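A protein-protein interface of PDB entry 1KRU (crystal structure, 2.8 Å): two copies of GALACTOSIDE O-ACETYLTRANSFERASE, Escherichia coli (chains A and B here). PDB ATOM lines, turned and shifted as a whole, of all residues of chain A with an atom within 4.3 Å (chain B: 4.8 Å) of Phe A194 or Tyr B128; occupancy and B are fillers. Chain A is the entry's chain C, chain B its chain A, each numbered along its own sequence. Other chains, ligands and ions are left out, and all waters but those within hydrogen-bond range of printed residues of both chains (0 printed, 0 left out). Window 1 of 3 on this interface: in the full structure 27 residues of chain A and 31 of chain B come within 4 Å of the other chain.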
ATOM      1  N   TYR A 192      18.963 -25.134  22.109  1.00  0.00           N
ATOM      2  CA  TYR A 192      18.103 -26.027  21.352  1.00  0.00           C
ATOM      3  C   TYR A 192      16.948 -25.230  20.807  1.00  0.00           C
ATOM      4  O   TYR A 192      16.078 -24.808  21.569  1.00  0.00           O
ATOM      5  CB  TYR A 192      17.569 -27.132  22.255  1.00  0.00           C
ATOM      6  CG  TYR A 192      18.522 -28.280  22.417  1.00  0.00           C
ATOM      7  CD1 TYR A 192      19.667 -28.156  23.213  1.00  0.00           C
ATOM      8  CD2 TYR A 192      18.305 -29.482  21.750  1.00  0.00           C
ATOM      9  CE1 TYR A 192      20.580 -29.211  23.330  1.00  0.00           C
ATOM     10  CE2 TYR A 192      19.206 -30.541  21.856  1.00  0.00           C
ATOM     11  CZ  TYR A 192      20.342 -30.400  22.646  1.00  0.00           C
ATOM     12  OH  TYR A 192      21.241 -31.435  22.745  1.00  0.00           O
ATOM     13  N   TYR A 193      16.928 -25.029  19.491  1.00  0.00           N
ATOM     14  CA  TYR A 193      15.854 -24.253  18.866  1.00  0.00           C
ATOM     15  C   TYR A 193      14.624 -25.049  18.435  1.00  0.00           C
ATOM     16  O   TYR A 193      13.528 -24.489  18.331  1.00  0.00           O
ATOM     17  CB  TYR A 193      16.379 -23.467  17.667  1.00  0.00           C
ATOM     18  CG  TYR A 193      17.092 -24.305  16.637  1.00  0.00           C
ATOM     19  CD1 TYR A 193      16.379 -25.077  15.711  1.00  0.00           C
ATOM     20  CD2 TYR A 193      18.479 -24.303  16.565  1.00  0.00           C
ATOM     21  CE1 TYR A 193      17.041 -25.818  14.742  1.00  0.00           C
ATOM     22  CE2 TYR A 193      19.148 -25.039  15.602  1.00  0.00           C
ATOM     23  CZ  TYR A 193      18.425 -25.790  14.694  1.00  0.00           C
ATOM     24  OH  TYR A 193      19.105 -26.497  13.738  1.00  0.00           O
ATOM     25  N   PHE A 194      14.794 -26.341  18.175  1.00  0.00           N
ATOM     26  CA  PHE A 194      13.659 -27.160  17.776  1.00  0.00           C
ATOM     27  C   PHE A 194      13.877 -28.629  18.063  1.00  0.00           C
ATOM     28  O   PHE A 194      14.702 -29.278  17.414  1.00  0.00           O
ATOM     29  CB  PHE A 194      13.353 -26.997  16.290  1.00  0.00           C
ATOM     30  CG  PHE A 194      12.378 -28.012  15.764  1.00  0.00           C
ATOM     31  CD1 PHE A 194      11.005 -27.858  15.983  1.00  0.00           C
ATOM     32  CD2 PHE A 194      12.824 -29.127  15.055  1.00  0.00           C
ATOM     33  CE1 PHE A 194      10.086 -28.804  15.500  1.00  0.00           C
ATOM     34  CE2 PHE A 194      11.921 -30.075  14.571  1.00  0.00           C
ATOM     35  CZ  PHE A 194      10.549 -29.914  14.793  1.00  0.00           C
ATOM     36  N   LYS A 195      13.123 -29.151  19.028  1.00  0.00           N
ATOM     37  CA  LYS A 195      13.233 -30.554  19.398  1.00  0.00           C
ATOM     38  C   LYS A 195      14.668 -30.900  19.783  1.00  0.00           C
ATOM     39  O   LYS A 195      15.173 -30.419  20.794  1.00  0.00           O
ATOM     40  CB  LYS A 195      12.785 -31.437  18.232  1.00  0.00           C
ATOM     41  CG  LYS A 195      11.374 -31.976  18.360  1.00  0.00           C
ATOM     42  CD  LYS A 195      10.788 -32.309  16.992  1.00  0.00           C
ATOM     43  CE  LYS A 195      11.641 -33.337  16.231  1.00  0.00           C
ATOM     44  NZ  LYS A 195      11.137 -33.591  14.837  1.00  0.00           N
ATOM     45  N   ASP A 196      15.327 -31.713  18.961  1.00  0.00           N
ATOM     46  CA  ASP A 196      16.698 -32.145  19.232  1.00  0.00           C
ATOM     47  C   ASP A 196      17.748 -31.488  18.359  1.00  0.00           C
ATOM     48  O   ASP A 196      18.848 -32.017  18.215  1.00  0.00           O
ATOM     49  CB  ASP A 196      16.813 -33.662  19.069  1.00  0.00           C
ATOM     50  CG  ASP A 196      15.872 -34.206  18.007  1.00  0.00           C
ATOM     51  OD1 ASP A 196      16.259 -34.261  16.818  1.00  0.00           O
ATOM     52  OD2 ASP A 196      14.734 -34.568  18.364  1.00  0.00           O
ATOM     53  N   TYR A 197      17.422 -30.348  17.763  1.00  0.00           N
ATOM     54  CA  TYR A 197      18.394 -29.661  16.917  1.00  0.00           C
ATOM     55  C   TYR A 197      19.002 -28.502  17.691  1.00  0.00           C
ATOM     56  O   TYR A 197      18.303 -27.569  18.063  1.00  0.00           O
ATOM     57  CB  TYR A 197      17.734 -29.148  15.632  1.00  0.00           C
ATOM     58  CG  TYR A 197      17.253 -30.243  14.701  1.00  0.00           C
ATOM     59  CD1 TYR A 197      16.069 -30.938  14.958  1.00  0.00           C
ATOM     60  CD2 TYR A 197      17.979 -30.575  13.554  1.00  0.00           C
ATOM     61  CE1 TYR A 197      15.617 -31.931  14.101  1.00  0.00           C
ATOM     62  CE2 TYR A 197      17.536 -31.570  12.687  1.00  0.00           C
ATOM     63  CZ  TYR A 197      16.352 -32.247  12.964  1.00  0.00           C
ATOM     64  OH  TYR A 197      15.892 -33.234  12.107  1.00  0.00           O
ATOM     65  N   LYS B  13      19.168 -25.894   9.659  1.00  0.00           N
ATOM     66  CA  LYS B  13      19.776 -24.848  10.457  1.00  0.00           C
ATOM     67  C   LYS B  13      18.905 -23.608  10.377  1.00  0.00           C
ATOM     68  O   LYS B  13      18.095 -23.476   9.455  1.00  0.00           O
ATOM     69  CB  LYS B  13      21.179 -24.554   9.936  1.00  0.00           C
ATOM     70  CG  LYS B  13      22.176 -25.616  10.340  1.00  0.00           C
ATOM     71  CD  LYS B  13      23.464 -25.526   9.554  1.00  0.00           C
ATOM     72  CE  LYS B  13      24.408 -26.639   9.976  1.00  0.00           C
ATOM     73  NZ  LYS B  13      25.841 -26.267   9.805  1.00  0.00           N
ATOM     74  N   LEU B  14      19.051 -22.712  11.352  1.00  0.00           N
ATOM     75  CA  LEU B  14      18.264 -21.486  11.350  1.00  0.00           C
ATOM     76  C   LEU B  14      18.716 -20.678  10.139  1.00  0.00           C
ATOM     77  O   LEU B  14      19.841 -20.839   9.667  1.00  0.00           O
ATOM     78  CB  LEU B  14      18.494 -20.691  12.637  1.00  0.00           C
ATOM     79  CG  LEU B  14      17.871 -21.298  13.892  1.00  0.00           C
ATOM     80  CD1 LEU B  14      18.416 -20.620  15.120  1.00  0.00           C
ATOM     81  CD2 LEU B  14      16.365 -21.147  13.829  1.00  0.00           C
ATOM     82  N   PHE B  15      17.839 -19.822   9.631  1.00  0.00           N
ATOM     83  CA  PHE B  15      18.162 -19.017   8.465  1.00  0.00           C
ATOM     84  C   PHE B  15      17.164 -17.874   8.319  1.00  0.00           C
ATOM     85  O   PHE B  15      16.154 -17.824   9.026  1.00  0.00           O
ATOM     86  CB  PHE B  15      18.123 -19.904   7.208  1.00  0.00           C
ATOM     87  CG  PHE B  15      16.726 -20.317   6.793  1.00  0.00           C
ATOM     88  CD1 PHE B  15      16.015 -19.566   5.858  1.00  0.00           C
ATOM     89  CD2 PHE B  15      16.097 -21.415   7.384  1.00  0.00           C
ATOM     90  CE1 PHE B  15      14.706 -19.896   5.525  1.00  0.00           C
ATOM     91  CE2 PHE B  15      14.782 -21.748   7.054  1.00  0.00           C
ATOM     92  CZ  PHE B  15      14.086 -20.987   6.125  1.00  0.00           C
ATOM     93  N   VAL B 112       5.962 -26.187   7.542  1.00  0.00           N
ATOM     94  CA  VAL B 112       7.262 -26.792   7.730  1.00  0.00           C
ATOM     95  C   VAL B 112       8.112 -25.866   8.597  1.00  0.00           C
ATOM     96  O   VAL B 112       9.041 -26.304   9.285  1.00  0.00           O
ATOM     97  CB  VAL B 112       7.954 -26.976   6.377  1.00  0.00           C
ATOM     98  CG1 VAL B 112       7.194 -27.971   5.562  1.00  0.00           C
ATOM     99  CG2 VAL B 112       8.007 -25.643   5.634  1.00  0.00           C
ATOM    100  N   THR B 113       7.762 -24.581   8.571  1.00  0.00           N
ATOM    101  CA  THR B 113       8.490 -23.553   9.296  1.00  0.00           C
ATOM    102  C   THR B 113       8.013 -23.203  10.699  1.00  0.00           C
ATOM    103  O   THR B 113       6.825 -23.234  11.013  1.00  0.00           O
ATOM    104  CB  THR B 113       8.526 -22.257   8.471  1.00  0.00           C
ATOM    105  OG1 THR B 113       9.243 -22.490   7.255  1.00  0.00           O
ATOM    106  CG2 THR B 113       9.206 -21.145   9.239  1.00  0.00           C
ATOM    107  N   GLY B 114       8.982 -22.845  11.528  1.00  0.00           N
ATOM    108  CA  GLY B 114       8.728 -22.450  12.901  1.00  0.00           C
ATOM    109  C   GLY B 114       9.851 -21.518  13.321  1.00  0.00           C
ATOM    110  O   GLY B 114      10.830 -21.322  12.588  1.00  0.00           O
ATOM    111  N   HIS B 115       9.720 -20.937  14.505  1.00  0.00           N
ATOM    112  CA  HIS B 115      10.738 -20.027  15.007  1.00  0.00           C
ATOM    113  C   HIS B 115      11.271 -20.493  16.351  1.00  0.00           C
ATOM    114  O   HIS B 115      10.570 -21.169  17.109  1.00  0.00           O
ATOM    115  CB  HIS B 115      10.167 -18.613  15.161  1.00  0.00           C
ATOM    116  CG  HIS B 115       9.669 -18.011  13.882  1.00  0.00           C
ATOM    117  ND1 HIS B 115      10.502 -17.387  12.986  1.00  0.00           N
ATOM    118  CD2 HIS B 115       8.418 -17.901  13.378  1.00  0.00           C
ATOM    119  CE1 HIS B 115       9.784 -16.912  11.979  1.00  0.00           C
ATOM    120  NE2 HIS B 115       8.519 -17.211  12.194  1.00  0.00           N
ATOM    121  N   PRO B 116      12.533 -20.157  16.656  1.00  0.00           N
ATOM    122  CA  PRO B 116      13.131 -20.553  17.937  1.00  0.00           C
ATOM    123  C   PRO B 116      12.324 -19.897  19.053  1.00  0.00           C
ATOM    124  O   PRO B 116      11.966 -18.717  18.978  1.00  0.00           O
ATOM    125  CB  PRO B 116      14.560 -20.017  17.867  1.00  0.00           C
ATOM    126  CG  PRO B 116      14.808 -19.781  16.421  1.00  0.00           C
ATOM    127  CD  PRO B 116      13.479 -19.410  15.816  1.00  0.00           C
ATOM    128  N   GLU B 126      14.659 -15.248  12.440  1.00  0.00           N
ATOM    129  CA  GLU B 126      15.340 -16.497  12.139  1.00  0.00           C
ATOM    130  C   GLU B 126      14.290 -17.573  12.155  1.00  0.00           C
ATOM    131  O   GLU B 126      13.326 -17.492  12.908  1.00  0.00           O
ATOM    132  CB  GLU B 126      16.393 -16.824  13.193  1.00  0.00           C
ATOM    133  CG  GLU B 126      17.760 -16.281  12.873  1.00  0.00           C
ATOM    134  CD  GLU B 126      18.012 -14.946  13.547  1.00  0.00           C
ATOM    135  OE1 GLU B 126      17.031 -14.274  13.937  1.00  0.00           O
ATOM    136  OE2 GLU B 126      19.193 -14.572  13.687  1.00  0.00           O
ATOM    137  N   MET B 127      14.465 -18.588  11.328  1.00  0.00           N
ATOM    138  CA  MET B 127      13.497 -19.663  11.300  1.00  0.00           C
ATOM    139  C   MET B 127      14.152 -20.979  10.917  1.00  0.00           C
ATOM    140  O   MET B 127      15.317 -21.032  10.509  1.00  0.00           O
ATOM    141  CB  MET B 127      12.369 -19.332  10.310  1.00  0.00           C
ATOM    142  CG  MET B 127      12.858 -18.907   8.930  1.00  0.00           C
ATOM    143  SD  MET B 127      11.620 -18.030   7.918  1.00  0.00           S
ATOM    144  CE  MET B 127      12.657 -17.034   6.885  1.00  0.00           C
ATOM    145  N   TYR B 128      13.387 -22.050  11.073  1.00  0.00           N
ATOM    146  CA  TYR B 128      13.864 -23.362  10.714  1.00  0.00           C
ATOM    147  C   TYR B 128      12.760 -23.995   9.904  1.00  0.00           C
ATOM    148  O   TYR B 128      11.589 -23.661  10.090  1.00  0.00           O
ATOM    149  CB  TYR B 128      14.149 -24.199  11.949  1.00  0.00           C
ATOM    150  CG  TYR B 128      13.051 -24.244  13.003  1.00  0.00           C
ATOM    151  CD1 TYR B 128      12.028 -25.194  12.907  1.00  0.00           C
ATOM    152  CD2 TYR B 128      13.088 -23.351  14.076  1.00  0.00           C
ATOM    153  CE1 TYR B 128      11.042 -25.255  13.897  1.00  0.00           C
ATOM    154  CE2 TYR B 128      12.104 -23.415  15.069  1.00  0.00           C
ATOM    155  CZ  TYR B 128      11.082 -24.369  14.980  1.00  0.00           C
ATOM    156  OH  TYR B 128      10.133 -24.435  15.950  1.00  0.00           O
ATOM    157  N   SER B 129      13.139 -24.901   9.006  1.00  0.00           N
ATOM    158  CA  SER B 129      12.175 -25.581   8.163  1.00  0.00           C
ATOM    159  C   SER B 129      12.424 -27.082   8.129  1.00  0.00           C
ATOM    160  O   SER B 129      13.535 -27.547   7.845  1.00  0.00           O
ATOM    161  CB  SER B 129      12.233 -25.002   6.755  1.00  0.00           C
ATOM    162  OG  SER B 129      11.395 -23.870   6.666  1.00  0.00           O
ATOM    163  N   PHE B 130      11.377 -27.840   8.427  1.00  0.00           N
ATOM    164  CA  PHE B 130      11.472 -29.295   8.435  1.00  0.00           C
ATOM    165  C   PHE B 130      10.337 -29.931   7.615  1.00  0.00           C
ATOM    166  O   PHE B 130       9.156 -29.831   7.960  1.00  0.00           O
ATOM    167  CB  PHE B 130      11.476 -29.807   9.884  1.00  0.00           C
ATOM    168  CG  PHE B 130      12.771 -29.556  10.616  1.00  0.00           C
ATOM    169  CD1 PHE B 130      12.869 -28.540  11.554  1.00  0.00           C
ATOM    170  CD2 PHE B 130      13.902 -30.320  10.347  1.00  0.00           C
ATOM    171  CE1 PHE B 130      14.076 -28.286  12.216  1.00  0.00           C
ATOM    172  CE2 PHE B 130      15.109 -30.068  11.005  1.00  0.00           C
ATOM    173  CZ  PHE B 130      15.191 -29.050  11.938  1.00  0.00           C
ATOM    174  N   PRO B 148       5.957 -28.461  11.837  1.00  0.00           N
ATOM    175  CA  PRO B 148       7.195 -28.896  11.169  1.00  0.00           C
ATOM    176  C   PRO B 148       7.692 -30.324  11.447  1.00  0.00           C
ATOM    177  O   PRO B 148       7.493 -30.865  12.536  1.00  0.00           O
ATOM    178  CB  PRO B 148       8.218 -27.843  11.600  1.00  0.00           C
ATOM    179  CG  PRO B 148       7.389 -26.631  11.885  1.00  0.00           C
ATOM    180  CD  PRO B 148       6.114 -27.143  12.480  1.00  0.00           C
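O of Val B112 is in hydrogen-bond range of N of Phe B130 (2.9 Å). The backbone carbonyl oxygen of Gly B114 lies within hydrogen-bond range of the backbone NH of Tyr B128 (3.1 Å). OH of Tyr B128 sits close to O of His B115.
CA of Lys B13 touches OH of Tyr A193, at 3.7 Å. CD1 of Leu B14 touches CD2 of Tyr A193, at 3.96 Å. Pro B116 touches Tyr A193 (CB to CB, 3.9 Å). Tyr A193 touches Tyr B128 (O to CE2, 3.7 Å). CE1 of Tyr B128 touches CD1 of Phe A194, at 3.3 Å. Phe B130 touches Phe A194. CZ of Phe A194 touches O of Pro B148, at 3.9 Å. Phe B130 touches Tyr A197 (CE2 to CZ, 3.2 Å).
Printed residues of chain B within 4 Å of Tyr A193: Lys B13, Leu B14, Pro B116 and Tyr B128. Of the printed residues of chain B, Tyr A197 touches Phe B130 (3.2 Å). Of the printed residues of chain A, Lys B13 touches Tyr A193 (3.7 Å). Gly B114 touches none of the printed residues of chain A. The nearest printed residue of chain B that does not touch Phe A194 is Pro B116 (6.0 Å). The nearest printed residue of chain A that does not touch Tyr B128 is Lys A195 (6.4 Å). The nearest printed residue of chain A that does not touch Leu B14 is Phe A194 (7.0 Å).
Of the 14 printed residues of chain B, 6 touch a printed residue of chain A. Hydrophobic or aromatic side chains of chain B that line the printed part of chain A: Leu B14, Pro B116, Tyr B128 and Phe B130. Hydrophobic or aromatic side chains of chain A within 4 Å of the printed part of chain B: Tyr A193, Phe A194 and Tyr A197. Among the printed residues, 8 pairs touch across the chains. Among the printed residues, no Asp or Glu carboxylate lies within 4 Å of a Lys or Arg side-chain nitrogen of the other chain.
No position is printed for both chains. Of the 8 pairs that touch across the chains among the printed residues, none has its exchanged pair printed and touching as well.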
